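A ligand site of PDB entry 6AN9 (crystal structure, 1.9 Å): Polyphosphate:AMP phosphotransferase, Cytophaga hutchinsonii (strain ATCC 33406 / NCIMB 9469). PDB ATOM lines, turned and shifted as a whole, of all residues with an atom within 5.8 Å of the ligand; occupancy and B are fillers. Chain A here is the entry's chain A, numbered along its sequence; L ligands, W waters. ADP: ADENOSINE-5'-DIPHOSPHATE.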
ATOM      1  N   ASP A  77      -6.712  -3.013 -37.290  1.00  0.00           N
ATOM      2  CA  ASP A  77      -6.996  -3.930 -38.417  1.00  0.00           C
ATOM      3  C   ASP A  77      -7.101  -3.186 -39.732  1.00  0.00           C
ATOM      4  O   ASP A  77      -7.575  -2.052 -39.796  1.00  0.00           O
ATOM      5  CB  ASP A  77      -8.288  -4.679 -38.188  1.00  0.00           C
ATOM      6  CG  ASP A  77      -8.206  -5.602 -37.004  1.00  0.00           C
ATOM      7  OD1 ASP A  77      -7.233  -6.401 -36.915  1.00  0.00           O
ATOM      8  OD2 ASP A  77      -9.088  -5.496 -36.141  1.00  0.00           O
ATOM      9  N   LYS A  81      -0.418  -3.758 -42.000  1.00  0.00           N
ATOM     10  CA  LYS A  81       0.712  -4.342 -41.275  1.00  0.00           C
ATOM     11  C   LYS A  81       1.263  -5.563 -41.978  1.00  0.00           C
ATOM     12  O   LYS A  81       2.464  -5.634 -42.275  1.00  0.00           O
ATOM     13  CB  LYS A  81       0.269  -4.733 -39.865  1.00  0.00           C
ATOM     14  CG  LYS A  81       1.380  -5.230 -38.999  1.00  0.00           C
ATOM     15  CD  LYS A  81       0.943  -5.450 -37.549  1.00  0.00           C
ATOM     16  CE  LYS A  81      -0.281  -6.366 -37.450  1.00  0.00           C
ATOM     17  NZ  LYS A  81      -0.172  -7.743 -38.112  1.00  0.00           N
ATOM     18  N   ASP A  82       0.427  -6.559 -42.197  1.00  0.00           N
ATOM     19  CA  ASP A  82       0.915  -7.824 -42.776  1.00  0.00           C
ATOM     20  C   ASP A  82       1.649  -7.567 -44.144  1.00  0.00           C
ATOM     21  O   ASP A  82       2.691  -8.119 -44.434  1.00  0.00           O
ATOM     22  CB  ASP A  82      -0.170  -8.978 -42.927  1.00  0.00           C
ATOM     23  CG  ASP A  82      -0.485  -9.756 -41.581  1.00  0.00           C
ATOM     24  OD1 ASP A  82      -1.344 -10.656 -41.567  1.00  0.00           O
ATOM     25  OD2 ASP A  82       0.142  -9.483 -40.536  1.00  0.00           O
ATOM     26  N   PHE A 102       2.784 -12.481 -33.089  1.00  0.00           N
ATOM     27  CA  PHE A 102       2.255 -12.834 -31.758  1.00  0.00           C
ATOM     28  C   PHE A 102       0.731 -12.822 -31.775  1.00  0.00           C
ATOM     29  O   PHE A 102       0.106 -11.862 -32.247  1.00  0.00           O
ATOM     30  CB  PHE A 102       2.787 -11.873 -30.694  1.00  0.00           C
ATOM     31  CG  PHE A 102       4.220 -12.162 -30.328  1.00  0.00           C
ATOM     32  CD1 PHE A 102       4.522 -13.266 -29.545  1.00  0.00           C
ATOM     33  CD2 PHE A 102       5.249 -11.424 -30.883  1.00  0.00           C
ATOM     34  CE1 PHE A 102       5.881 -13.540 -29.232  1.00  0.00           C
ATOM     35  CE2 PHE A 102       6.557 -11.713 -30.582  1.00  0.00           C
ATOM     36  CZ  PHE A 102       6.892 -12.766 -29.775  1.00  0.00           C
ATOM     37  N   LYS A 103       0.149 -13.936 -31.313  1.00  0.00           N
ATOM     38  CA  LYS A 103      -1.307 -14.125 -31.303  1.00  0.00           C
ATOM     39  C   LYS A 103      -1.815 -14.201 -29.894  1.00  0.00           C
ATOM     40  O   LYS A 103      -1.075 -13.961 -28.952  1.00  0.00           O
ATOM     41  CB  LYS A 103      -1.641 -15.461 -31.998  1.00  0.00           C
ATOM     42  CG  LYS A 103      -0.890 -15.749 -33.267  1.00  0.00           C
ATOM     43  CD  LYS A 103      -1.317 -14.868 -34.349  1.00  0.00           C
ATOM     44  CE  LYS A 103      -0.737 -15.268 -35.737  1.00  0.00           C
ATOM     45  NZ  LYS A 103      -1.183 -14.182 -36.704  1.00  0.00           N
ATOM     46  N   VAL A 104      -3.058 -14.722 -29.741  1.00  0.00           N
ATOM     47  CA  VAL A 104      -3.579 -14.822 -28.376  1.00  0.00           C
ATOM     48  C   VAL A 104      -2.670 -15.741 -27.580  1.00  0.00           C
ATOM     49  O   VAL A 104      -2.333 -16.828 -28.058  1.00  0.00           O
ATOM     50  CB  VAL A 104      -5.032 -15.337 -28.367  1.00  0.00           C
ATOM     51  CG1 VAL A 104      -5.457 -15.651 -27.014  1.00  0.00           C
ATOM     52  CG2 VAL A 104      -5.997 -14.273 -29.005  1.00  0.00           C
ATOM     53  N   PRO A 105      -2.300 -15.418 -26.343  1.00  0.00           N
ATOM     54  CA  PRO A 105      -1.385 -16.293 -25.604  1.00  0.00           C
ATOM     55  C   PRO A 105      -1.928 -17.695 -25.389  1.00  0.00           C
ATOM     56  O   PRO A 105      -3.126 -17.921 -25.102  1.00  0.00           O
ATOM     57  CB  PRO A 105      -1.190 -15.550 -24.267  1.00  0.00           C
ATOM     58  CG  PRO A 105      -1.406 -14.109 -24.618  1.00  0.00           C
ATOM     59  CD  PRO A 105      -2.489 -14.097 -25.657  1.00  0.00           C
ATOM     60  N   ARG A 117       7.192 -14.398 -23.255  1.00  0.00           N
ATOM     61  CA  ARG A 117       7.210 -14.965 -24.601  1.00  0.00           C
ATOM     62  C   ARG A 117       7.955 -14.051 -25.558  1.00  0.00           C
ATOM     63  O   ARG A 117       8.457 -14.508 -26.597  1.00  0.00           O
ATOM     64  CB  ARG A 117       5.798 -15.222 -25.099  1.00  0.00           C
ATOM     65  CG  ARG A 117       4.911 -14.056 -25.353  1.00  0.00           C
ATOM     66  CD  ARG A 117       3.415 -14.515 -25.696  1.00  0.00           C
ATOM     67  NE  ARG A 117       2.615 -13.371 -26.150  1.00  0.00           N
ATOM     68  CZ  ARG A 117       1.610 -13.518 -27.029  1.00  0.00           C
ATOM     69  NH1 ARG A 117       1.286 -14.762 -27.470  1.00  0.00           N
ATOM     70  NH2 ARG A 117       0.970 -12.450 -27.460  1.00  0.00           N
ATOM     71  N   HIS A 118       8.020 -12.768 -25.258  1.00  0.00           N
ATOM     72  CA  HIS A 118       8.794 -11.841 -26.075  1.00  0.00           C
ATOM     73  C   HIS A 118      10.274 -11.950 -25.802  1.00  0.00           C
ATOM     74  O   HIS A 118      11.093 -12.019 -26.714  1.00  0.00           O
ATOM     75  CB  HIS A 118       8.246 -10.403 -25.842  1.00  0.00           C
ATOM     76  CG  HIS A 118       6.804 -10.295 -26.149  1.00  0.00           C
ATOM     77  ND1 HIS A 118       6.334 -10.381 -27.434  1.00  0.00           N
ATOM     78  CD2 HIS A 118       5.703 -10.352 -25.365  1.00  0.00           C
ATOM     79  CE1 HIS A 118       5.031 -10.387 -27.441  1.00  0.00           C
ATOM     80  NE2 HIS A 118       4.605 -10.336 -26.194  1.00  0.00           N
ATOM     81  N   ASN A 132       5.809  -8.935 -35.320  1.00  0.00           N
ATOM     82  CA  ASN A 132       4.548  -8.609 -35.963  1.00  0.00           C
ATOM     83  C   ASN A 132       3.435  -8.716 -34.910  1.00  0.00           C
ATOM     84  O   ASN A 132       2.985  -9.798 -34.583  1.00  0.00           O
ATOM     85  CB  ASN A 132       4.320  -9.581 -37.130  1.00  0.00           C
ATOM     86  CG  ASN A 132       2.991  -9.359 -37.871  1.00  0.00           C
ATOM     87  OD1 ASN A 132       2.433  -8.298 -37.832  1.00  0.00           O
ATOM     88  ND2 ASN A 132       2.534 -10.379 -38.563  1.00  0.00           N
ATOM     89  N   ARG A 133       3.085  -7.573 -34.323  1.00  0.00           N
ATOM     90  CA  ARG A 133       2.517  -7.499 -32.968  1.00  0.00           C
ATOM     91  C   ARG A 133       3.581  -7.892 -31.942  1.00  0.00           C
ATOM     92  O   ARG A 133       4.587  -8.490 -32.309  1.00  0.00           O
ATOM     93  CB  ARG A 133       1.292  -8.327 -32.760  1.00  0.00           C
ATOM     94  CG  ARG A 133       0.154  -7.984 -33.680  1.00  0.00           C
ATOM     95  CD  ARG A 133      -1.128  -8.744 -33.290  1.00  0.00           C
ATOM     96  NE  ARG A 133      -2.202  -8.522 -34.261  1.00  0.00           N
ATOM     97  CZ  ARG A 133      -3.082  -7.534 -34.217  1.00  0.00           C
ATOM     98  NH1 ARG A 133      -3.067  -6.644 -33.208  1.00  0.00           N
ATOM     99  NH2 ARG A 133      -4.027  -7.491 -35.161  1.00  0.00           N
ATOM    100  N   SER A 134       3.394  -7.489 -30.678  1.00  0.00           N
ATOM    101  CA  SER A 134       4.529  -7.418 -29.775  1.00  0.00           C
ATOM    102  C   SER A 134       4.044  -7.444 -28.341  1.00  0.00           C
ATOM    103  O   SER A 134       2.838  -7.524 -28.058  1.00  0.00           O
ATOM    104  CB  SER A 134       5.337  -6.166 -30.035  1.00  0.00           C
ATOM    105  OG  SER A 134       4.639  -5.031 -29.567  1.00  0.00           O
ATOM    106  N   GLU A 137       0.927  -5.425 -27.126  1.00  0.00           N
ATOM    107  CA  GLU A 137      -0.442  -5.894 -27.074  1.00  0.00           C
ATOM    108  C   GLU A 137      -0.976  -5.802 -25.664  1.00  0.00           C
ATOM    109  O   GLU A 137      -2.185  -5.618 -25.508  1.00  0.00           O
ATOM    110  CB  GLU A 137      -0.586  -7.363 -27.594  1.00  0.00           C
ATOM    111  CG  GLU A 137      -0.319  -7.439 -29.115  1.00  0.00           C
ATOM    112  CD  GLU A 137      -1.511  -6.950 -29.973  1.00  0.00           C
ATOM    113  OE1 GLU A 137      -2.693  -7.202 -29.605  1.00  0.00           O
ATOM    114  OE2 GLU A 137      -1.272  -6.370 -31.050  1.00  0.00           O
ATOM    115  N   ASN A 138      -0.099  -5.939 -24.654  1.00  0.00           N
ATOM    116  CA  ASN A 138      -0.466  -5.986 -23.254  1.00  0.00           C
ATOM    117  C   ASN A 138      -0.782  -4.610 -22.692  1.00  0.00           C
ATOM    118  O   ASN A 138      -1.132  -4.518 -21.517  1.00  0.00           O
ATOM    119  CB  ASN A 138       0.675  -6.663 -22.490  1.00  0.00           C
ATOM    120  CG  ASN A 138       0.837  -8.119 -22.942  1.00  0.00           C
ATOM    121  OD1 ASN A 138      -0.062  -8.917 -22.673  1.00  0.00           O
ATOM    122  ND2 ASN A 138       1.883  -8.431 -23.698  1.00  0.00           N
ATOM    123  N   VAL A 141      -4.970  -4.318 -26.739  1.00  0.00           N
ATOM    124  CA  VAL A 141      -6.183  -5.176 -26.786  1.00  0.00           C
ATOM    125  C   VAL A 141      -6.600  -5.491 -25.307  1.00  0.00           C
ATOM    126  O   VAL A 141      -7.748  -5.377 -24.974  1.00  0.00           O
ATOM    127  CB  VAL A 141      -6.055  -6.506 -27.632  1.00  0.00           C
ATOM    128  CG1 VAL A 141      -4.870  -7.345 -27.210  1.00  0.00           C
ATOM    129  CG2 VAL A 141      -7.345  -7.284 -27.657  1.00  0.00           C
ATOM    130  N   THR A 142      -5.655  -5.878 -24.421  1.00  0.00           N
ATOM    131  CA  THR A 142      -5.975  -6.144 -22.986  1.00  0.00           C
ATOM    132  C   THR A 142      -6.447  -4.831 -22.193  1.00  0.00           C
ATOM    133  O   THR A 142      -7.071  -4.964 -21.157  1.00  0.00           O
ATOM    134  CB  THR A 142      -4.851  -6.888 -22.168  1.00  0.00           C
ATOM    135  OG1 THR A 142      -3.752  -6.023 -22.032  1.00  0.00           O
ATOM    136  CG2 THR A 142      -4.396  -8.198 -22.920  1.00  0.00           C
ATOM    137  N   TYR A 148      -9.540  -9.865 -20.544  1.00  0.00           N
ATOM    138  CA  TYR A 148      -8.437 -10.747 -20.880  1.00  0.00           C
ATOM    139  C   TYR A 148      -7.419 -10.831 -19.739  1.00  0.00           C
ATOM    140  O   TYR A 148      -6.699 -11.843 -19.626  1.00  0.00           O
ATOM    141  CB  TYR A 148      -7.783 -10.245 -22.173  1.00  0.00           C
ATOM    142  CG  TYR A 148      -8.776 -10.205 -23.386  1.00  0.00           C
ATOM    143  CD1 TYR A 148     -10.093 -10.733 -23.288  1.00  0.00           C
ATOM    144  CD2 TYR A 148      -8.387  -9.671 -24.606  1.00  0.00           C
ATOM    145  CE1 TYR A 148     -10.988 -10.687 -24.384  1.00  0.00           C
ATOM    146  CE2 TYR A 148      -9.233  -9.644 -25.700  1.00  0.00           C
ATOM    147  CZ  TYR A 148     -10.559 -10.141 -25.601  1.00  0.00           C
ATOM    148  OH  TYR A 148     -11.434 -10.114 -26.692  1.00  0.00           O
ATOM    149  N   GLU A 152      -4.870 -14.119 -17.433  1.00  0.00           N
ATOM    150  CA  GLU A 152      -3.457 -13.983 -17.181  1.00  0.00           C
ATOM    151  C   GLU A 152      -3.254 -14.333 -15.716  1.00  0.00           C
ATOM    152  O   GLU A 152      -3.539 -13.522 -14.818  1.00  0.00           O
ATOM    153  CB  GLU A 152      -3.009 -12.578 -17.485  1.00  0.00           C
ATOM    154  CG  GLU A 152      -3.103 -12.252 -18.961  1.00  0.00           C
ATOM    155  CD  GLU A 152      -2.708 -10.848 -19.302  1.00  0.00           C
ATOM    156  OE1 GLU A 152      -1.894 -10.231 -18.560  1.00  0.00           O
ATOM    157  OE2 GLU A 152      -3.230 -10.351 -20.338  1.00  0.00           O
ATOM    158  N   TYR A 232      -9.275   2.316 -28.385  1.00  0.00           N
ATOM    159  CA  TYR A 232      -7.952   2.036 -28.909  1.00  0.00           C
ATOM    160  C   TYR A 232      -7.137   3.300 -29.068  1.00  0.00           C
ATOM    161  O   TYR A 232      -5.945   3.317 -28.793  1.00  0.00           O
ATOM    162  CB  TYR A 232      -8.025   1.281 -30.220  1.00  0.00           C
ATOM    163  CG  TYR A 232      -8.202  -0.214 -30.034  1.00  0.00           C
ATOM    164  CD1 TYR A 232      -7.139  -1.033 -29.650  1.00  0.00           C
ATOM    165  CD2 TYR A 232      -9.404  -0.816 -30.300  1.00  0.00           C
ATOM    166  CE1 TYR A 232      -7.284  -2.348 -29.493  1.00  0.00           C
ATOM    167  CE2 TYR A 232      -9.581  -2.136 -30.159  1.00  0.00           C
ATOM    168  CZ  TYR A 232      -8.498  -2.928 -29.786  1.00  0.00           C
ATOM    169  OH  TYR A 232      -8.622  -4.278 -29.608  1.00  0.00           O
HETATM  170  PB  ADP L   1      -2.895 -10.289 -37.486  1.00  0.00           P
HETATM  171  O1B ADP L   1      -4.130  -9.486 -37.294  1.00  0.00           O
HETATM  172  O2B ADP L   1      -2.536 -10.615 -38.903  1.00  0.00           O
HETATM  173  O3B ADP L   1      -1.670  -9.709 -36.730  1.00  0.00           O
HETATM  174  PA  ADP L   1      -4.486 -12.435 -36.240  1.00  0.00           P
HETATM  175  O1A ADP L   1      -5.642 -12.230 -37.231  1.00  0.00           O
HETATM  176  O2A ADP L   1      -3.976 -13.812 -36.016  1.00  0.00           O
HETATM  177  O3A ADP L   1      -3.148 -11.670 -36.678  1.00  0.00           O
HETATM  178  O5' ADP L   1      -4.898 -11.878 -34.788  1.00  0.00           O
HETATM  179  C5' ADP L   1      -3.972 -11.969 -33.669  1.00  0.00           C
HETATM  180  C4' ADP L   1      -4.773 -11.623 -32.416  1.00  0.00           C
HETATM  181  O4' ADP L   1      -4.018 -11.921 -31.250  1.00  0.00           O
HETATM  182  C3' ADP L   1      -5.122 -10.175 -32.348  1.00  0.00           C
HETATM  183  O3' ADP L   1      -6.548 -10.095 -32.121  1.00  0.00           O
HETATM  184  C2' ADP L   1      -4.290  -9.705 -31.149  1.00  0.00           C
HETATM  185  O2' ADP L   1      -4.908  -8.584 -30.526  1.00  0.00           O
HETATM  186  C1' ADP L   1      -4.222 -10.957 -30.238  1.00  0.00           C
HETATM  187  N9  ADP L   1      -3.123 -10.819 -29.290  1.00  0.00           N
HETATM  188  C8  ADP L   1      -1.825 -10.690 -29.553  1.00  0.00           C
HETATM  189  N7  ADP L   1      -1.162 -10.521 -28.404  1.00  0.00           N
HETATM  190  C5  ADP L   1      -2.070 -10.609 -27.425  1.00  0.00           C
HETATM  191  C6  ADP L   1      -2.042 -10.528 -25.990  1.00  0.00           C
HETATM  192  N6  ADP L   1      -0.853 -10.299 -25.382  1.00  0.00           N
HETATM  193  N1  ADP L   1      -3.212 -10.683 -25.317  1.00  0.00           N
HETATM  194  C2  ADP L   1      -4.369 -10.897 -25.910  1.00  0.00           C
HETATM  195  N3  ADP L   1      -4.511 -10.938 -27.255  1.00  0.00           N
HETATM  196  C4  ADP L   1      -3.355 -10.804 -27.994  1.00  0.00           C
HETATM  197  O   HOH W   1      -2.068  -7.474 -40.279  1.00  0.00           O
HETATM  198  O   HOH W   2       0.145 -11.633 -35.439  1.00  0.00           O
HETATM  199  O   HOH W   3       1.857  -9.836 -26.646  1.00  0.00           O
HETATM  200  O   HOH W   4      -5.128 -15.551 -34.617  1.00  0.00           O
HETATM  201  O   HOH W   5      -4.593  -6.939 -38.190  1.00  0.00           O
HETATM  202  O   HOH W   6      -3.009 -11.568 -22.502  1.00  0.00           O
HETATM  203  O   HOH W   7      -6.492  -5.554 -31.252  1.00  0.00           O
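The side-chain amino group (NZ) of Lys 81 lies within salt-bridge range of an oxygen (O3B) of the ligand, 2.8 Å away.
An oxygen (O3B) of the ligand lies within salt-bridge range of the guanidinium group (NE) of Arg 133, 2.8 Å away.
The backbone NH of Val 104 is in hydrogen-bond range of an oxygen (O4') of the ligand.
The side-chain amino group (NZ) of Lys 103 lies within salt-bridge range of an oxygen (O2A) of the ligand, at 2.9 Å.
The side-chain amide oxygen of Asn 138 lies within hydrogen-bond range of a nitrogen (N6) of the ligand.
The side-chain carboxylate of Glu 137 lies within hydrogen-bond range of an oxygen (O2') of the ligand (2.8 Å).
An oxygen (O2B) of the ligand sits close to the side-chain carboxylate of Asp 82 (2.9 Å).
The guanidinium group of Arg 117 lies within hydrogen-bond range of a nitrogen (N7) of the ligand (3.0 Å).
OE2 of Glu 137 is in salt-bridge range of NH1 of Arg 133, 2.8 Å away.
OG1 of Thr 142 is in hydrogen-bond range of O of Asn 138 (3.1 Å).
The guanidinium group of Arg 133 is in salt-bridge range of the side-chain carboxylate of Asp 77 (3.8 Å).
The side-chain carboxylate (OD2) of Asp 82 lies within salt-bridge range of the side-chain amino group (NZ) of Lys 81 (3.0 Å).
ND2 of Asn 132 is in hydrogen-bond range of OD2 of Asp 82.
The side-chain amide oxygen (OD1) of Asn 132 sits at hydrogen-bond distance from the side-chain amino group (NZ) of Lys 81.
The backbone NH of Phe 102 lies within hydrogen-bond range of the backbone carbonyl oxygen of Asn 132, at 3.1 Å.
The guanidinium group (NH1) of Arg 117 lies within hydrogen-bond range of the backbone carbonyl oxygen (O) of Lys 103 (2.9 Å).
Phe 102 touches the ligand.
Pro 105 touches the ligand (CD to N1, 3.5 Å).
Val 141 touches the ligand.
CG2 of Thr 142 touches N1 of the ligand (3.7 Å).
Hydrophobic or aromatic side chains that line the ligand: Val 104, Pro 105 and Val 141.
Of the 19 residues printed, 12 come within 4 Å of the ligand.
The nearest printed residue that does not touch the ligand is Asp 77 (4.4 Å).
Water W5 lies within hydrogen-bond range of O1B of the ligand (2.7 Å), OD1 of Asp 77 (3.0 Å) and NH2 of Arg 133 (3.1 Å).
Water W2 lies within hydrogen-bond range of O3B of the ligand, NZ of Lys 103, O of Phe 102 and O of Asn 132.
Water W6 lies within hydrogen-bond range of OE2 of Glu 152 (2.5 Å) and N1 of the ligand (3.0 Å).
Water W1 lies within hydrogen-bond range of the side-chain amino group (NZ) of Lys 81 (2.9 Å), the side-chain carboxylate (OD2) of Asp 82 (3.0 Å) and an oxygen (O2B) of the ligand (3.5 Å).
Water W7 bridges OH of Tyr 232 (3.0 Å) and O2' of the ligand (3.5 Å).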
